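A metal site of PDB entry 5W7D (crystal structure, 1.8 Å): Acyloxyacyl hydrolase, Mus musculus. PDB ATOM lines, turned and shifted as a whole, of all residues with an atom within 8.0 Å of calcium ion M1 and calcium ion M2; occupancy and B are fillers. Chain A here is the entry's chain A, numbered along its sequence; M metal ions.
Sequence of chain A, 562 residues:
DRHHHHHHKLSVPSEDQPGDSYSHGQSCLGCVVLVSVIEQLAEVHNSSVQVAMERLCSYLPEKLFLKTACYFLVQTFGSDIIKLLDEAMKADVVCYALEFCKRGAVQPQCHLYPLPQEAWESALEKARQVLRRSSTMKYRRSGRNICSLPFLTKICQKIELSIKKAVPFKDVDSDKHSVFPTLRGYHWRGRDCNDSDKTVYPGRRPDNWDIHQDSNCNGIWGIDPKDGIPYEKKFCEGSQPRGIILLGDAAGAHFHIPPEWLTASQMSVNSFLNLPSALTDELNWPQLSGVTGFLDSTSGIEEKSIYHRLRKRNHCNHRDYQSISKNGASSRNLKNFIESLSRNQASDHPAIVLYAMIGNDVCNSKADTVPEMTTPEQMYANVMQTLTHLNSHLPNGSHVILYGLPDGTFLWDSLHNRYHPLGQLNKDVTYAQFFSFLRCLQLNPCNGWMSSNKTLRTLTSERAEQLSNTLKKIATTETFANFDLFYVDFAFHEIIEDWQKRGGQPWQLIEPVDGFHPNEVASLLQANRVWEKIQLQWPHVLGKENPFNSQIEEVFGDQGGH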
ATOM      1  N   PRO A 168      -9.683   9.871  -2.477  1.00  0.00           N
ATOM      2  CA  PRO A 168      -9.059   9.655  -1.160  1.00  0.00           C
ATOM      3  C   PRO A 168      -9.364   8.289  -0.627  1.00  0.00           C
ATOM      4  O   PRO A 168     -10.463   7.755  -0.784  1.00  0.00           O
ATOM      5  CB  PRO A 168      -9.662  10.743  -0.276  1.00  0.00           C
ATOM      6  CG  PRO A 168     -10.884  11.184  -0.978  1.00  0.00           C
ATOM      7  CD  PRO A 168     -10.629  10.996  -2.443  1.00  0.00           C
ATOM      8  N   LYS A 170      -9.120   7.604   2.679  1.00  0.00           N
ATOM      9  CA  LYS A 170      -9.933   7.870   3.862  1.00  0.00           C
ATOM     10  C   LYS A 170     -11.107   8.769   3.463  1.00  0.00           C
ATOM     11  O   LYS A 170     -10.918   9.951   3.175  1.00  0.00           O
ATOM     12  CB  LYS A 170      -9.105   8.552   4.951  1.00  0.00           C
ATOM     13  CG  LYS A 170      -7.888   7.759   5.413  1.00  0.00           C
ATOM     14  CD  LYS A 170      -8.319   6.671   6.384  1.00  0.00           C
ATOM     15  CE  LYS A 170      -7.123   5.995   7.037  1.00  0.00           C
ATOM     16  NZ  LYS A 170      -7.495   4.688   7.688  1.00  0.00           N
ATOM     17  N   ASP A 171     -12.307   8.203   3.448  1.00  0.00           N
ATOM     18  CA  ASP A 171     -13.469   8.922   2.939  1.00  0.00           C
ATOM     19  C   ASP A 171     -14.702   8.102   3.277  1.00  0.00           C
ATOM     20  O   ASP A 171     -15.243   7.381   2.445  1.00  0.00           O
ATOM     21  CB  ASP A 171     -13.318   9.167   1.442  1.00  0.00           C
ATOM     22  CG  ASP A 171     -14.518   9.897   0.816  1.00  0.00           C
ATOM     23  OD1 ASP A 171     -15.321  10.528   1.532  1.00  0.00           O
ATOM     24  OD2 ASP A 171     -14.637   9.841  -0.426  1.00  0.00           O
ATOM     25  N   VAL A 172     -15.148   8.215   4.528  1.00  0.00           N
ATOM     26  CA  VAL A 172     -16.149   7.288   5.047  1.00  0.00           C
ATOM     27  C   VAL A 172     -17.449   7.389   4.256  1.00  0.00           C
ATOM     28  O   VAL A 172     -18.076   6.375   3.961  1.00  0.00           O
ATOM     29  CB  VAL A 172     -16.368   7.550   6.548  1.00  0.00           C
ATOM     30  CG1 VAL A 172     -17.618   6.784   7.069  1.00  0.00           C
ATOM     31  CG2 VAL A 172     -15.099   7.139   7.308  1.00  0.00           C
ATOM     32  N   ASP A 173     -17.850   8.608   3.855  1.00  0.00           N
ATOM     33  CA  ASP A 173     -19.118   8.814   3.172  1.00  0.00           C
ATOM     34  C   ASP A 173     -18.995   8.842   1.658  1.00  0.00           C
ATOM     35  O   ASP A 173     -20.003   9.040   0.981  1.00  0.00           O
ATOM     36  CB  ASP A 173     -19.795  10.119   3.673  1.00  0.00           C
ATOM     37  CG  ASP A 173     -18.979  11.377   3.407  1.00  0.00           C
ATOM     38  OD1 ASP A 173     -18.015  11.305   2.620  1.00  0.00           O
ATOM     39  OD2 ASP A 173     -19.322  12.432   3.984  1.00  0.00           O
ATOM     40  N   SER A 174     -17.798   8.620   1.119  1.00  0.00           N
ATOM     41  CA  SER A 174     -17.575   8.430  -0.302  1.00  0.00           C
ATOM     42  C   SER A 174     -17.916   9.660  -1.144  1.00  0.00           C
ATOM     43  O   SER A 174     -18.283   9.519  -2.315  1.00  0.00           O
ATOM     44  CB  SER A 174     -18.346   7.223  -0.837  1.00  0.00           C
ATOM     45  OG  SER A 174     -17.915   6.065  -0.172  1.00  0.00           O
ATOM     46  N   ASP A 175     -17.777  10.867  -0.606  1.00  0.00           N
ATOM     47  CA  ASP A 175     -18.036  12.052  -1.415  1.00  0.00           C
ATOM     48  C   ASP A 175     -16.765  12.653  -2.006  1.00  0.00           C
ATOM     49  O   ASP A 175     -16.815  13.758  -2.555  1.00  0.00           O
ATOM     50  CB  ASP A 175     -18.825  13.101  -0.616  1.00  0.00           C
ATOM     51  CG  ASP A 175     -18.081  13.617   0.593  1.00  0.00           C
ATOM     52  OD1 ASP A 175     -16.859  13.401   0.748  1.00  0.00           O
ATOM     53  OD2 ASP A 175     -18.766  14.256   1.401  1.00  0.00           O
ATOM     54  N   LYS A 176     -15.644  11.942  -1.905  1.00  0.00           N
ATOM     55  CA  LYS A 176     -14.349  12.290  -2.477  1.00  0.00           C
ATOM     56  C   LYS A 176     -13.649  13.423  -1.733  1.00  0.00           C
ATOM     57  O   LYS A 176     -12.601  13.856  -2.172  1.00  0.00           O
ATOM     58  CB  LYS A 176     -14.456  12.654  -3.957  1.00  0.00           C
ATOM     59  CG  LYS A 176     -15.096  11.547  -4.789  1.00  0.00           C
ATOM     60  CD  LYS A 176     -15.112  11.876  -6.232  1.00  0.00           C
ATOM     61  CE  LYS A 176     -15.373  10.642  -7.072  1.00  0.00           C
ATOM     62  NZ  LYS A 176     -16.732  10.123  -6.819  1.00  0.00           N
ATOM     63  N   HIS A 177     -14.170  13.862  -0.589  1.00  0.00           N
ATOM     64  CA  HIS A 177     -13.462  14.800   0.281  1.00  0.00           C
ATOM     65  C   HIS A 177     -13.112  14.107   1.599  1.00  0.00           C
ATOM     66  O   HIS A 177     -13.902  13.345   2.131  1.00  0.00           O
ATOM     67  CB  HIS A 177     -14.321  16.052   0.545  1.00  0.00           C
ATOM     68  CG  HIS A 177     -14.599  16.857  -0.673  1.00  0.00           C
ATOM     69  ND1 HIS A 177     -13.842  17.954  -1.029  1.00  0.00           N
ATOM     70  CD2 HIS A 177     -15.498  16.678  -1.659  1.00  0.00           C
ATOM     71  CE1 HIS A 177     -14.295  18.450  -2.164  1.00  0.00           C
ATOM     72  NE2 HIS A 177     -15.305  17.700  -2.573  1.00  0.00           N
ATOM     73  N   SER A 178     -11.929  14.420   2.126  1.00  0.00           N
ATOM     74  CA  SER A 178     -11.331  13.677   3.239  1.00  0.00           C
ATOM     75  C   SER A 178     -11.099  14.576   4.439  1.00  0.00           C
ATOM     76  O   SER A 178     -11.056  15.810   4.321  1.00  0.00           O
ATOM     77  CB  SER A 178      -9.993  13.060   2.772  1.00  0.00           C
ATOM     78  OG  SER A 178      -9.423  12.172   3.725  1.00  0.00           O
ATOM     79  N   VAL A 179     -10.919  13.945   5.609  1.00  0.00           N
ATOM     80  CA  VAL A 179     -10.404  14.649   6.767  1.00  0.00           C
ATOM     81  C   VAL A 179      -8.923  14.417   6.968  1.00  0.00           C
ATOM     82  O   VAL A 179      -8.345  14.993   7.895  1.00  0.00           O
ATOM     83  CB  VAL A 179     -11.184  14.287   8.053  1.00  0.00           C
ATOM     84  CG1 VAL A 179     -12.688  14.572   7.833  1.00  0.00           C
ATOM     85  CG2 VAL A 179     -10.883  12.856   8.528  1.00  0.00           C
ATOM     86  N   GLY A 190     -10.851  20.489  -1.000  1.00  0.00           N
ATOM     87  CA  GLY A 190     -11.309  20.987   0.284  1.00  0.00           C
ATOM     88  C   GLY A 190     -11.621  19.910   1.293  1.00  0.00           C
ATOM     89  O   GLY A 190     -12.205  18.862   0.959  1.00  0.00           O
ATOM     90  N   ARG A 191     -11.181  20.127   2.524  1.00  0.00           N
ATOM     91  CA  ARG A 191     -11.443  19.201   3.596  1.00  0.00           C
ATOM     92  C   ARG A 191     -12.942  19.032   3.844  1.00  0.00           C
ATOM     93  O   ARG A 191     -13.699  20.011   3.884  1.00  0.00           O
ATOM     94  CB  ARG A 191     -10.748  19.688   4.858  1.00  0.00           C
ATOM     95  CG  ARG A 191     -10.840  18.732   6.015  1.00  0.00           C
ATOM     96  CD  ARG A 191     -10.443  19.336   7.336  1.00  0.00           C
ATOM     97  NE  ARG A 191      -9.116  19.936   7.412  1.00  0.00           N
ATOM     98  CZ  ARG A 191      -8.143  19.576   8.255  1.00  0.00           C
ATOM     99  NH1 ARG A 191      -8.285  18.561   9.094  1.00  0.00           N
ATOM    100  NH2 ARG A 191      -6.999  20.245   8.255  1.00  0.00           N
ATOM    101  N   ASP A 192     -13.347  17.788   4.070  1.00  0.00           N
ATOM    102  CA  ASP A 192     -14.717  17.435   4.416  1.00  0.00           C
ATOM    103  C   ASP A 192     -15.024  17.862   5.843  1.00  0.00           C
ATOM    104  O   ASP A 192     -14.415  17.343   6.799  1.00  0.00           O
ATOM    105  CB  ASP A 192     -14.908  15.914   4.259  1.00  0.00           C
ATOM    106  CG  ASP A 192     -16.353  15.490   4.125  1.00  0.00           C
ATOM    107  OD1 ASP A 192     -17.219  16.330   4.387  1.00  0.00           O
ATOM    108  OD2 ASP A 192     -16.598  14.309   3.723  1.00  0.00           O
ATOM    109  N   CYS A 193     -16.010  18.743   6.003  1.00  0.00           N
ATOM    110  CA  CYS A 193     -16.434  19.158   7.347  1.00  0.00           C
ATOM    111  C   CYS A 193     -17.332  18.122   8.012  1.00  0.00           C
ATOM    112  O   CYS A 193     -17.460  18.118   9.248  1.00  0.00           O
ATOM    113  CB  CYS A 193     -17.113  20.548   7.266  1.00  0.00           C
ATOM    114  SG  CYS A 193     -18.560  20.731   6.104  1.00  0.00           S
ATOM    115  N   ASN A 194     -17.913  17.183   7.252  1.00  0.00           N
ATOM    116  CA  ASN A 194     -18.666  16.088   7.853  1.00  0.00           C
ATOM    117  C   ASN A 194     -18.495  14.846   6.974  1.00  0.00           C
ATOM    118  O   ASN A 194     -19.156  14.708   5.962  1.00  0.00           O
ATOM    119  CB  ASN A 194     -20.124  16.463   8.024  1.00  0.00           C
ATOM    120  CG  ASN A 194     -20.877  15.472   8.844  1.00  0.00           C
ATOM    121  OD1 ASN A 194     -20.493  14.298   8.966  1.00  0.00           O
ATOM    122  ND2 ASN A 194     -21.978  15.933   9.411  1.00  0.00           N
ATOM    123  N   ASP A 195     -17.584  13.982   7.380  1.00  0.00           N
ATOM    124  CA  ASP A 195     -17.278  12.776   6.628  1.00  0.00           C
ATOM    125  C   ASP A 195     -18.281  11.646   6.880  1.00  0.00           C
ATOM    126  O   ASP A 195     -18.077  10.547   6.349  1.00  0.00           O
ATOM    127  CB  ASP A 195     -15.848  12.344   6.977  1.00  0.00           C
ATOM    128  CG  ASP A 195     -15.260  11.377   5.984  1.00  0.00           C
ATOM    129  OD1 ASP A 195     -15.548  11.464   4.769  1.00  0.00           O
ATOM    130  OD2 ASP A 195     -14.460  10.524   6.419  1.00  0.00           O
ATOM    131  N   SER A 196     -19.355  11.908   7.650  1.00  0.00           N
ATOM    132  CA  SER A 196     -20.501  11.016   7.807  1.00  0.00           C
ATOM    133  C   SER A 196     -21.742  11.478   7.038  1.00  0.00           C
ATOM    134  O   SER A 196     -22.858  11.067   7.377  1.00  0.00           O
ATOM    135  CB  SER A 196     -20.867  10.879   9.280  1.00  0.00           C
ATOM    136  OG  SER A 196     -19.760  10.495  10.033  1.00  0.00           O
ATOM    137  N   ASP A 197     -21.589  12.362   6.057  1.00  0.00           N
ATOM    138  CA  ASP A 197     -22.734  12.870   5.322  1.00  0.00           C
ATOM    139  C   ASP A 197     -22.291  13.213   3.916  1.00  0.00           C
ATOM    140  O   ASP A 197     -21.622  14.235   3.702  1.00  0.00           O
ATOM    141  CB  ASP A 197     -23.349  14.081   6.021  1.00  0.00           C
ATOM    142  CG  ASP A 197     -24.671  14.494   5.407  1.00  0.00           C
ATOM    143  OD1 ASP A 197     -24.916  14.155   4.227  1.00  0.00           O
ATOM    144  OD2 ASP A 197     -25.476  15.148   6.101  1.00  0.00           O
ATOM    145  N   LYS A 198     -22.693  12.386   2.954  1.00  0.00           N
ATOM    146  CA  LYS A 198     -22.270  12.544   1.581  1.00  0.00           C
ATOM    147  C   LYS A 198     -22.894  13.754   0.898  1.00  0.00           C
ATOM    148  O   LYS A 198     -22.524  14.045  -0.254  1.00  0.00           O
ATOM    149  CB  LYS A 198     -22.620  11.274   0.779  1.00  0.00           C
ATOM    150  CG  LYS A 198     -24.126  11.000   0.697  1.00  0.00           C
ATOM    151  CD  LYS A 198     -24.407   9.786  -0.189  1.00  0.00           C
ATOM    152  CE  LYS A 198     -25.902   9.486  -0.217  1.00  0.00           C
ATOM    153  NZ  LYS A 198     -26.247   8.323  -1.100  1.00  0.00           N
ATOM    154  N   THR A 199     -23.830  14.449   1.557  1.00  0.00           N
ATOM    155  CA  THR A 199     -24.398  15.672   1.014  1.00  0.00           C
ATOM    156  C   THR A 199     -23.772  16.921   1.626  1.00  0.00           C
ATOM    157  O   THR A 199     -24.229  18.031   1.350  1.00  0.00           O
ATOM    158  CB  THR A 199     -25.929  15.725   1.216  1.00  0.00           C
ATOM    159  OG1 THR A 199     -26.220  15.875   2.617  1.00  0.00           O
ATOM    160  CG2 THR A 199     -26.587  14.471   0.679  1.00  0.00           C
ATOM    161  N   VAL A 200     -22.760  16.760   2.455  1.00  0.00           N
ATOM    162  CA  VAL A 200     -22.004  17.860   3.070  1.00  0.00           C
ATOM    163  C   VAL A 200     -20.584  17.771   2.517  1.00  0.00           C
ATOM    164  O   VAL A 200     -19.866  16.819   2.825  1.00  0.00           O
ATOM    165  CB  VAL A 200     -22.004  17.776   4.600  1.00  0.00           C
ATOM    166  CG1 VAL A 200     -21.023  18.781   5.213  1.00  0.00           C
ATOM    167  CG2 VAL A 200     -23.430  17.976   5.130  1.00  0.00           C
ATOM    168  N   TYR A 201     -20.163  18.779   1.752  1.00  0.00           N
ATOM    169  CA  TYR A 201     -18.831  18.846   1.165  1.00  0.00           C
ATOM    170  C   TYR A 201     -18.654  20.218   0.513  1.00  0.00           C
ATOM    171  O   TYR A 201     -19.646  20.881   0.187  1.00  0.00           O
ATOM    172  CB  TYR A 201     -18.624  17.731   0.124  1.00  0.00           C
ATOM    173  CG  TYR A 201     -19.679  17.691  -0.960  1.00  0.00           C
ATOM    174  CD1 TYR A 201     -19.624  18.560  -2.037  1.00  0.00           C
ATOM    175  CD2 TYR A 201     -20.731  16.781  -0.912  1.00  0.00           C
ATOM    176  CE1 TYR A 201     -20.584  18.553  -3.016  1.00  0.00           C
ATOM    177  CE2 TYR A 201     -21.689  16.760  -1.887  1.00  0.00           C
ATOM    178  CZ  TYR A 201     -21.616  17.644  -2.945  1.00  0.00           C
ATOM    179  OH  TYR A 201     -22.584  17.619  -3.911  1.00  0.00           O
ATOM    180  N   PRO A 202     -17.409  20.628   0.262  1.00  0.00           N
ATOM    181  CA  PRO A 202     -17.158  21.928  -0.392  1.00  0.00           C
ATOM    182  C   PRO A 202     -17.700  21.986  -1.810  1.00  0.00           C
ATOM    183  O   PRO A 202     -17.569  21.038  -2.589  1.00  0.00           O
ATOM    184  CB  PRO A 202     -15.632  22.041  -0.367  1.00  0.00           C
ATOM    185  CG  PRO A 202     -15.190  21.079   0.673  1.00  0.00           C
ATOM    186  CD  PRO A 202     -16.158  19.962   0.652  1.00  0.00           C
ATOM    187  N   GLN A 213     -26.571  23.533   9.989  1.00  0.00           N
ATOM    188  CA  GLN A 213     -25.333  22.853   9.681  1.00  0.00           C
ATOM    189  C   GLN A 213     -24.649  23.605   8.543  1.00  0.00           C
ATOM    190  O   GLN A 213     -25.313  24.171   7.666  1.00  0.00           O
ATOM    191  CB  GLN A 213     -25.510  21.367   9.274  1.00  0.00           C
ATOM    192  CG  GLN A 213     -24.190  20.735   8.744  1.00  0.00           C
ATOM    193  CD  GLN A 213     -24.111  19.176   8.723  1.00  0.00           C
ATOM    194  OE1 GLN A 213     -23.030  18.584   8.939  1.00  0.00           O
ATOM    195  NE2 GLN A 213     -25.249  18.522   8.418  1.00  0.00           N
ATOM    196  N   SER A 215     -23.419  23.086   5.528  1.00  0.00           N
ATOM    197  CA  SER A 215     -23.526  22.007   4.552  1.00  0.00           C
ATOM    198  C   SER A 215     -22.504  22.103   3.434  1.00  0.00           C
ATOM    199  O   SER A 215     -22.242  21.092   2.779  1.00  0.00           O
ATOM    200  CB  SER A 215     -24.931  21.942   3.947  1.00  0.00           C
ATOM    201  OG  SER A 215     -25.171  23.006   3.023  1.00  0.00           O
ATOM    202  N   CYS A 217     -19.299  23.519   3.880  1.00  0.00           N
ATOM    203  CA  CYS A 217     -17.960  23.527   4.456  1.00  0.00           C
ATOM    204  C   CYS A 217     -17.240  24.866   4.264  1.00  0.00           C
ATOM    205  O   CYS A 217     -15.995  24.933   4.413  1.00  0.00           O
ATOM    206  CB  CYS A 217     -17.101  22.394   3.883  1.00  0.00           C
ATOM    207  SG  CYS A 217     -17.885  20.765   4.088  1.00  0.00           S
HETATM  208 CA    CA M   1     -15.925  12.414   2.675  1.00  0.00          CA
HETATM  209 CA    CA M   2     -19.115  14.748   3.619  1.00  0.00          CA
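Of the 27 residues printed, 6 come within 4 Å of calcium ion M1.
The nearest printed residue that does not touch calcium ion M1 is Ser 178 (4.5 Å).
The backbone NH of Ser 174 lies close to the side-chain carboxylate of Asp 171 (3.2 Å).
The backbone NH of Asp 192 is in hydrogen-bond range of the backbone carbonyl oxygen of Ser 178.
The backbone NH (N) of Val 172 sits at hydrogen-bond distance from the side-chain carboxylate (OD2) of Asp 195 (3.1 Å).
OD1 of Asp 197 is in hydrogen-bond range of OG1 of Thr 199, at 2.7 Å.
SG of Cys 193 forms a disulfide with SG of Cys 217 (2.1 Å).
O of Gly 190 sits at hydrogen-bond distance from ND1 of His 177 (2.7 Å).
ND2 of Asn 194 is in hydrogen-bond range of OE1 of Gln 213 (2.9 Å).
OD2 of Asp 171 lies within hydrogen-bond range of N of Lys 176 (2.8 Å).
The side-chain carboxylate (OD2) of Asp 175 is bound to calcium ion M2 (2.3 Å).
O of Val 200 binds calcium ion M2, 2.3 Å away.
O of Asn 194 binds calcium ion M2 (2.3 Å).
Calcium ion M2 is bound by the side-chain carboxylate (OD2) of Asp 173.
OD2 of Asp 192 is bound to calcium ion M2 (2.6 Å).
The backbone carbonyl oxygen (O) of Asp 197 is bound to calcium ion M2.
The side-chain carboxylate (OD1) of Asp 192 binds calcium ion M2 (2.6 Å).
Calcium ion M1 is bound by the side-chain carboxylate of Asp 192 (2.3 Å), the side-chain carboxylate of Asp 171 (2.3 Å), the backbone carbonyl oxygen of His 177 (2.3 Å), the side-chain carboxylate of Asp 195 (2.3 Å), the side-chain carboxylate of Asp 175 (2.4 Å) and the side-chain carboxylate of Asp 173 (2.4 Å).
Calcium ion M1 has six donor atoms within binding distance.
Six residues have an atom within 4 Å of calcium ion M2: Asp 173, Asp 175, Asp 192, Asn 194, Asp 197 and Val 200.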
